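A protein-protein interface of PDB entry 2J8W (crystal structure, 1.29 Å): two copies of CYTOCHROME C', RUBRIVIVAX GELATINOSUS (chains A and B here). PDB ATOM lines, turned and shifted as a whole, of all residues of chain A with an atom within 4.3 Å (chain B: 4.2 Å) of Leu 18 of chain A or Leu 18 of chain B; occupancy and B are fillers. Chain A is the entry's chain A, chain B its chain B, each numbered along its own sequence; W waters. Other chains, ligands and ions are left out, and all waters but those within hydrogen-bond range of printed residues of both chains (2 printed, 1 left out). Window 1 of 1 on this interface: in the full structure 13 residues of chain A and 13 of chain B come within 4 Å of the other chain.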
ATOM      1  N   TYR A  11      10.638  -2.555  33.010  1.00  0.00           N
ATOM      2  CA  TYR A  11       9.492  -1.759  32.525  1.00  0.00           C
ATOM      3  C   TYR A  11       9.966  -0.498  31.861  1.00  0.00           C
ATOM      4  O   TYR A  11       9.544  -0.184  30.746  1.00  0.00           O
ATOM      5  CB  TYR A  11       8.621  -1.422  33.718  1.00  0.00           C
ATOM      6  CG  TYR A  11       7.405  -0.579  33.404  1.00  0.00           C
ATOM      7  CD1 TYR A  11       6.163  -1.172  33.195  1.00  0.00           C
ATOM      8  CD2 TYR A  11       7.480   0.799  33.387  1.00  0.00           C
ATOM      9  CE1 TYR A  11       5.010  -0.393  32.947  1.00  0.00           C
ATOM     10  CE2 TYR A  11       6.345   1.583  33.145  1.00  0.00           C
ATOM     11  CZ  TYR A  11       5.140   0.988  32.905  1.00  0.00           C
ATOM     12  OH  TYR A  11       4.044   1.778  32.668  1.00  0.00           O
ATOM     13  N   SER A  14      11.720  -1.238  28.589  1.00  0.00           N
ATOM     14  CA  SER A  14      10.729  -1.649  27.600  1.00  0.00           C
ATOM     15  C   SER A  14       9.983  -0.440  27.048  1.00  0.00           C
ATOM     16  O   SER A  14       9.780  -0.336  25.837  1.00  0.00           O
ATOM     17  CB  SER A  14       9.766  -2.625  28.259  1.00  0.00           C
ATOM     18  OG  SER A  14      10.398  -3.859  28.571  1.00  0.00           O
ATOM     19  N   ALA A  15       9.525   0.465  27.910  1.00  0.00           N
ATOM     20  CA  ALA A  15       8.847   1.643  27.418  1.00  0.00           C
ATOM     21  C   ALA A  15       9.738   2.481  26.530  1.00  0.00           C
ATOM     22  O   ALA A  15       9.293   2.951  25.476  1.00  0.00           O
ATOM     23  CB  ALA A  15       8.269   2.446  28.562  1.00  0.00           C
ATOM     24  N   PHE A  16      10.986   2.697  26.926  1.00  0.00           N
ATOM     25  CA  PHE A  16      11.906   3.458  26.080  1.00  0.00           C
ATOM     26  C   PHE A  16      12.131   2.803  24.731  1.00  0.00           C
ATOM     27  O   PHE A  16      12.206   3.504  23.742  1.00  0.00           O
ATOM     28  CB  PHE A  16      13.244   3.686  26.782  1.00  0.00           C
ATOM     29  CG  PHE A  16      13.207   4.743  27.858  1.00  0.00           C
ATOM     30  CD1 PHE A  16      12.715   6.005  27.625  1.00  0.00           C
ATOM     31  CD2 PHE A  16      13.667   4.453  29.139  1.00  0.00           C
ATOM     32  CE1 PHE A  16      12.707   6.981  28.648  1.00  0.00           C
ATOM     33  CE2 PHE A  16      13.688   5.413  30.155  1.00  0.00           C
ATOM     34  CZ  PHE A  16      13.206   6.660  29.924  1.00  0.00           C
ATOM     35  N   THR A  17      12.227   1.479  24.693  1.00  0.00           N
ATOM     36  CA  THR A  17      12.373   0.788  23.410  1.00  0.00           C
ATOM     37  C   THR A  17      11.178   1.046  22.491  1.00  0.00           C
ATOM     38  O   THR A  17      11.333   1.361  21.328  1.00  0.00           O
ATOM     39  CB  THR A  17      12.581  -0.706  23.617  1.00  0.00           C
ATOM     40  OG1 THR A  17      13.854  -0.909  24.231  1.00  0.00           O
ATOM     41  CG2 THR A  17      12.503  -1.523  22.352  1.00  0.00           C
ATOM     42  N   LEU A  18       9.964   0.950  23.038  1.00  0.00           N
ATOM     43  CA  LEU A  18       8.783   1.207  22.205  1.00  0.00           C
ATOM     44  C   LEU A  18       8.713   2.662  21.773  1.00  0.00           C
ATOM     45  O   LEU A  18       8.374   2.956  20.614  1.00  0.00           O
ATOM     46  CB  LEU A  18       7.521   0.792  22.946  1.00  0.00           C
ATOM     47  CG  LEU A  18       7.391  -0.692  23.317  1.00  0.00           C
ATOM     48  CD1 LEU A  18       5.988  -0.929  23.847  1.00  0.00           C
ATOM     49  CD2 LEU A  18       7.608  -1.658  22.235  1.00  0.00           C
ATOM     50  N   ILE A  19       9.048   3.590  22.673  1.00  0.00           N
ATOM     51  CA  ILE A  19       9.079   5.001  22.329  1.00  0.00           C
ATOM     52  C   ILE A  19      10.060   5.232  21.194  1.00  0.00           C
ATOM     53  O   ILE A  19       9.738   5.924  20.209  1.00  0.00           O
ATOM     54  CB  ILE A  19       9.460   5.851  23.564  1.00  0.00           C
ATOM     55  CG1 ILE A  19       8.330   5.843  24.592  1.00  0.00           C
ATOM     56  CG2 ILE A  19       9.858   7.284  23.148  1.00  0.00           C
ATOM     57  CD1 ILE A  19       8.763   6.349  25.966  1.00  0.00           C
ATOM     58  N   ALA A  20      11.270   4.670  21.319  1.00  0.00           N
ATOM     59  CA  ALA A  20      12.267   4.905  20.281  1.00  0.00           C
ATOM     60  C   ALA A  20      11.802   4.374  18.935  1.00  0.00           C
ATOM     61  O   ALA A  20      12.020   5.017  17.901  1.00  0.00           O
ATOM     62  CB  ALA A  20      13.588   4.245  20.693  1.00  0.00           C
ATOM     63  N   ASN A  21      11.159   3.212  18.929  1.00  0.00           N
ATOM     64  CA  ASN A  21      10.736   2.652  17.653  1.00  0.00           C
ATOM     65  C   ASN A  21       9.665   3.531  16.991  1.00  0.00           C
ATOM     66  O   ASN A  21       9.770   3.905  15.818  1.00  0.00           O
ATOM     67  CB  ASN A  21      10.239   1.240  17.831  1.00  0.00           C
ATOM     68  CG  ASN A  21       9.893   0.625  16.549  1.00  0.00           C
ATOM     69  OD1 ASN A  21       8.826   0.854  16.009  1.00  0.00           O
ATOM     70  ND2 ASN A  21      10.851  -0.125  15.982  1.00  0.00           N
ATOM     71  N   HIS A  22       8.640   3.907  17.728  1.00  0.00           N
ATOM     72  CA  HIS A  22       7.569   4.694  17.127  1.00  0.00           C
ATOM     73  C   HIS A  22       7.988   6.124  16.842  1.00  0.00           C
ATOM     74  O   HIS A  22       7.608   6.674  15.807  1.00  0.00           O
ATOM     75  CB  HIS A  22       6.306   4.569  17.997  1.00  0.00           C
ATOM     76  CG  HIS A  22       5.700   3.222  17.884  1.00  0.00           C
ATOM     77  ND1 HIS A  22       4.932   2.862  16.791  1.00  0.00           N
ATOM     78  CD2 HIS A  22       5.874   2.094  18.604  1.00  0.00           C
ATOM     79  CE1 HIS A  22       4.628   1.571  16.894  1.00  0.00           C
ATOM     80  NE2 HIS A  22       5.179   1.085  17.991  1.00  0.00           N
ATOM     81  N   LEU A  51       2.963   6.378  25.412  1.00  0.00           N
ATOM     82  CA  LEU A  51       4.107   5.696  26.016  1.00  0.00           C
ATOM     83  C   LEU A  51       5.000   6.612  26.823  1.00  0.00           C
ATOM     84  O   LEU A  51       5.626   6.176  27.798  1.00  0.00           O
ATOM     85  CB  LEU A  51       4.925   5.003  24.921  1.00  0.00           C
ATOM     86  CG  LEU A  51       4.289   3.841  24.156  1.00  0.00           C
ATOM     87  CD1 LEU A  51       5.024   3.601  22.847  1.00  0.00           C
ATOM     88  CD2 LEU A  51       4.246   2.593  25.009  1.00  0.00           C
ATOM     89  N   TYR B  11      11.592  -5.395  20.558  1.00  0.00           N
ATOM     90  CA  TYR B  11      10.319  -4.685  20.532  1.00  0.00           C
ATOM     91  C   TYR B  11       9.211  -5.557  21.100  1.00  0.00           C
ATOM     92  O   TYR B  11       8.425  -5.106  21.932  1.00  0.00           O
ATOM     93  CB  TYR B  11      10.020  -4.249  19.102  1.00  0.00           C
ATOM     94  CG  TYR B  11       8.721  -3.524  18.897  1.00  0.00           C
ATOM     95  CD1 TYR B  11       8.684  -2.156  18.825  1.00  0.00           C
ATOM     96  CD2 TYR B  11       7.540  -4.221  18.693  1.00  0.00           C
ATOM     97  CE1 TYR B  11       7.474  -1.483  18.595  1.00  0.00           C
ATOM     98  CE2 TYR B  11       6.339  -3.564  18.452  1.00  0.00           C
ATOM     99  CZ  TYR B  11       6.332  -2.197  18.401  1.00  0.00           C
ATOM    100  OH  TYR B  11       5.149  -1.567  18.149  1.00  0.00           O
ATOM    101  N   SER B  14       9.554  -6.098  24.799  1.00  0.00           N
ATOM    102  CA  SER B  14       9.247  -4.865  25.493  1.00  0.00           C
ATOM    103  C   SER B  14       7.745  -4.670  25.588  1.00  0.00           C
ATOM    104  O   SER B  14       7.217  -4.306  26.653  1.00  0.00           O
ATOM    105  CB  SER B  14       9.865  -3.696  24.764  1.00  0.00           C
ATOM    106  OG  SER B  14      11.294  -3.711  24.897  1.00  0.00           O
ATOM    107  N   ALA B  15       7.023  -4.877  24.489  1.00  0.00           N
ATOM    108  CA  ALA B  15       5.584  -4.727  24.513  1.00  0.00           C
ATOM    109  C   ALA B  15       4.934  -5.733  25.463  1.00  0.00           C
ATOM    110  O   ALA B  15       4.028  -5.360  26.220  1.00  0.00           O
ATOM    111  CB  ALA B  15       5.019  -4.794  23.102  1.00  0.00           C
ATOM    112  N   PHE B  16       5.376  -6.990  25.439  1.00  0.00           N
ATOM    113  CA  PHE B  16       4.819  -7.976  26.343  1.00  0.00           C
ATOM    114  C   PHE B  16       5.087  -7.612  27.815  1.00  0.00           C
ATOM    115  O   PHE B  16       4.215  -7.804  28.674  1.00  0.00           O
ATOM    116  CB  PHE B  16       5.340  -9.377  26.056  1.00  0.00           C
ATOM    117  CG  PHE B  16       4.767 -10.013  24.819  1.00  0.00           C
ATOM    118  CD1 PHE B  16       3.408 -10.162  24.680  1.00  0.00           C
ATOM    119  CD2 PHE B  16       5.594 -10.547  23.832  1.00  0.00           C
ATOM    120  CE1 PHE B  16       2.874 -10.795  23.573  1.00  0.00           C
ATOM    121  CE2 PHE B  16       5.046 -11.183  22.722  1.00  0.00           C
ATOM    122  CZ  PHE B  16       3.723 -11.282  22.601  1.00  0.00           C
ATOM    123  N   THR B  17       6.251  -7.075  28.121  1.00  0.00           N
ATOM    124  CA  THR B  17       6.554  -6.624  29.472  1.00  0.00           C
ATOM    125  C   THR B  17       5.550  -5.551  29.943  1.00  0.00           C
ATOM    126  O   THR B  17       5.027  -5.617  31.038  1.00  0.00           O
ATOM    127  CB  THR B  17       7.990  -6.132  29.570  1.00  0.00           C
ATOM    128  OG1 THR B  17       8.835  -7.271  29.418  1.00  0.00           O
ATOM    129  CG2 THR B  17       8.256  -5.473  30.927  1.00  0.00           C
ATOM    130  N   LEU B  18       5.316  -4.559  29.103  1.00  0.00           N
ATOM    131  CA  LEU B  18       4.371  -3.502  29.476  1.00  0.00           C
ATOM    132  C   LEU B  18       2.956  -4.019  29.615  1.00  0.00           C
ATOM    133  O   LEU B  18       2.233  -3.641  30.540  1.00  0.00           O
ATOM    134  CB  LEU B  18       4.410  -2.351  28.487  1.00  0.00           C
ATOM    135  CG  LEU B  18       5.784  -1.655  28.352  1.00  0.00           C
ATOM    136  CD1 LEU B  18       5.593  -0.494  27.376  1.00  0.00           C
ATOM    137  CD2 LEU B  18       6.295  -1.138  29.664  1.00  0.00           C
ATOM    138  N   ILE B  19       2.566  -4.892  28.698  1.00  0.00           N
ATOM    139  CA  ILE B  19       1.250  -5.550  28.758  1.00  0.00           C
ATOM    140  C   ILE B  19       1.092  -6.261  30.091  1.00  0.00           C
ATOM    141  O   ILE B  19       0.066  -6.117  30.785  1.00  0.00           O
ATOM    142  CB  ILE B  19       1.016  -6.517  27.568  1.00  0.00           C
ATOM    143  CG1 ILE B  19       0.857  -5.744  26.273  1.00  0.00           C
ATOM    144  CG2 ILE B  19      -0.171  -7.426  27.833  1.00  0.00           C
ATOM    145  CD1 ILE B  19       1.030  -6.569  25.013  1.00  0.00           C
ATOM    146  N   ALA B  20       2.099  -7.065  30.457  1.00  0.00           N
ATOM    147  CA  ALA B  20       2.025  -7.845  31.687  1.00  0.00           C
ATOM    148  C   ALA B  20       1.885  -6.947  32.895  1.00  0.00           C
ATOM    149  O   ALA B  20       1.102  -7.214  33.826  1.00  0.00           O
ATOM    150  CB  ALA B  20       3.256  -8.746  31.829  1.00  0.00           C
ATOM    151  N   ASN B  21       2.619  -5.856  32.910  1.00  0.00           N
ATOM    152  CA  ASN B  21       2.555  -4.990  34.068  1.00  0.00           C
ATOM    153  C   ASN B  21       1.179  -4.336  34.224  1.00  0.00           C
ATOM    154  O   ASN B  21       0.576  -4.376  35.303  1.00  0.00           O
ATOM    155  CB  ASN B  21       3.627  -3.935  34.042  1.00  0.00           C
ATOM    156  CG  ASN B  21       3.623  -3.116  35.287  1.00  0.00           C
ATOM    157  OD1 ASN B  21       2.857  -2.157  35.386  1.00  0.00           O
ATOM    158  ND2 ASN B  21       4.476  -3.477  36.266  1.00  0.00           N
ATOM    159  N   HIS B  22       0.672  -3.749  33.150  1.00  0.00           N
ATOM    160  CA  HIS B  22      -0.621  -3.063  33.244  1.00  0.00           C
ATOM    161  C   HIS B  22      -1.758  -4.038  33.436  1.00  0.00           C
ATOM    162  O   HIS B  22      -2.707  -3.740  34.169  1.00  0.00           O
ATOM    163  CB  HIS B  22      -0.785  -2.110  32.061  1.00  0.00           C
ATOM    164  CG  HIS B  22       0.107  -0.929  32.193  1.00  0.00           C
ATOM    165  ND1 HIS B  22      -0.212   0.112  33.031  1.00  0.00           N
ATOM    166  CD2 HIS B  22       1.343  -0.663  31.731  1.00  0.00           C
ATOM    167  CE1 HIS B  22       0.793   0.982  33.038  1.00  0.00           C
ATOM    168  NE2 HIS B  22       1.759   0.522  32.268  1.00  0.00           N
ATOM    169  N   LEU B  51      -1.473  -1.503  23.717  1.00  0.00           N
ATOM    170  CA  LEU B  51      -0.247  -2.274  23.654  1.00  0.00           C
ATOM    171  C   LEU B  51      -0.454  -3.610  22.969  1.00  0.00           C
ATOM    172  O   LEU B  51       0.461  -4.138  22.331  1.00  0.00           O
ATOM    173  CB  LEU B  51       0.335  -2.486  25.050  1.00  0.00           C
ATOM    174  CG  LEU B  51       0.861  -1.235  25.735  1.00  0.00           C
ATOM    175  CD1 LEU B  51       1.007  -1.497  27.249  1.00  0.00           C
ATOM    176  CD2 LEU B  51       2.225  -0.784  25.171  1.00  0.00           C
HETATM  177  O   HOH W   1      14.334  -2.806  26.015  1.00  0.00           O
HETATM  178  O   HOH W   2      12.834  -4.911  27.256  1.00  0.00           O
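A ring nitrogen (NE2) of His 22 of chain B lies within hydrogen-bond range of the side-chain hydroxyl of Tyr 11 of chain A, at 2.6 Å. NE2 of His 22 of chain A is in hydrogen-bond range of OH of Tyr 11 of chain B (2.7 Å).
Among the printed residues, merely in contact across the chains: Ser 14 of chain A with Ser 14 of chain B, Ser 14 of chain A with Thr 17 of chain B, Thr 17 of chain A with Ser 14 of chain B, Tyr 11 of chain A with Leu 18 of chain B, Leu 18 of chain A with Tyr 11 of chain B, Leu 18 of chain A with Leu 18 of chain B, Tyr 11 of chain A with Asn 21 of chain B, Asn 21 of chain A with Tyr 11 of chain B, Leu 18 of chain A with Ala 15 of chain B, Ala 15 of chain A with Leu 18 of chain B, Leu 51 of chain A with Leu 51 of chain B, Leu 18 of chain A with Ser 14 of chain B and Leu 18 of chain A with Leu 51 of chain B.
Phe 16 of chain A touches none of the printed residues of chain B. Of the printed residues of chain B, Leu 18 of chain A touches Tyr 11 (3.6 Å), Ser 14 (3.96 Å), Ala 15 (3.9 Å), Leu 18 (3.6 Å) and Leu 51 (3.99 Å). Printed residues of chain B within 4 Å of His 22 of chain A: Tyr 11. Of the printed residues of chain A, Thr 17 of chain B touches Ser 14. Leu 18 of chain B touches just these residues of chain A: Tyr 11 (3.5 Å), Ala 15 (3.9 Å) and Leu 18 (3.6 Å). Of the printed residues of chain A, His 22 of chain B touches Tyr 11. Printed residues of chain A within 4 Å of Leu 51 of chain B: Leu 18 and Leu 51. The nearest residue of chain A that does not touch Leu 18 of chain B is Ser 14 of chain A (4.03 Å).
Of the 11 printed residues of chain A, 8 touch a printed residue of chain B. Printed residues of chain B that touch a printed residue of chain A: Tyr 11, Ser 14, Ala 15, Thr 17, Leu 18, Asn 21, His 22 and Leu 51. Among the printed residues, 15 pairs touch across the chains.
Tyr 11 of chain A touches Asn 21 of chain B, and with the chains exchanged Asn 21 of chain A touches Tyr 11 of chain B. Tyr 11 of chain A touches His 22 of chain B, and with the chains exchanged His 22 of chain A touches Tyr 11 of chain B. Ala 15 of chain A touches Leu 18 of chain B, and with the chains exchanged Leu 18 of chain A touches Ala 15 of chain B. Leu 51 of chain B touches its own counterpart, Leu 51 of chain A. Positions printed for both chains: 11, 14, 15, 16, 17, 18, 19, 20, 21, 22 and 51. Of the 15 pairs that touch across the chains among the printed residues, 13 have their exchanged pair printed and touching as well.
Water W1 bridges the side-chain hydroxyl (OG1) of Thr 17 of chain A and the side-chain hydroxyl (OG) of Ser 14 of chain B. Water W2 lies within hydrogen-bond range of the side-chain hydroxyl of Ser 14 of chain A (3.0 Å) and the side-chain hydroxyl of Ser 14 of chain B (3.1 Å).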
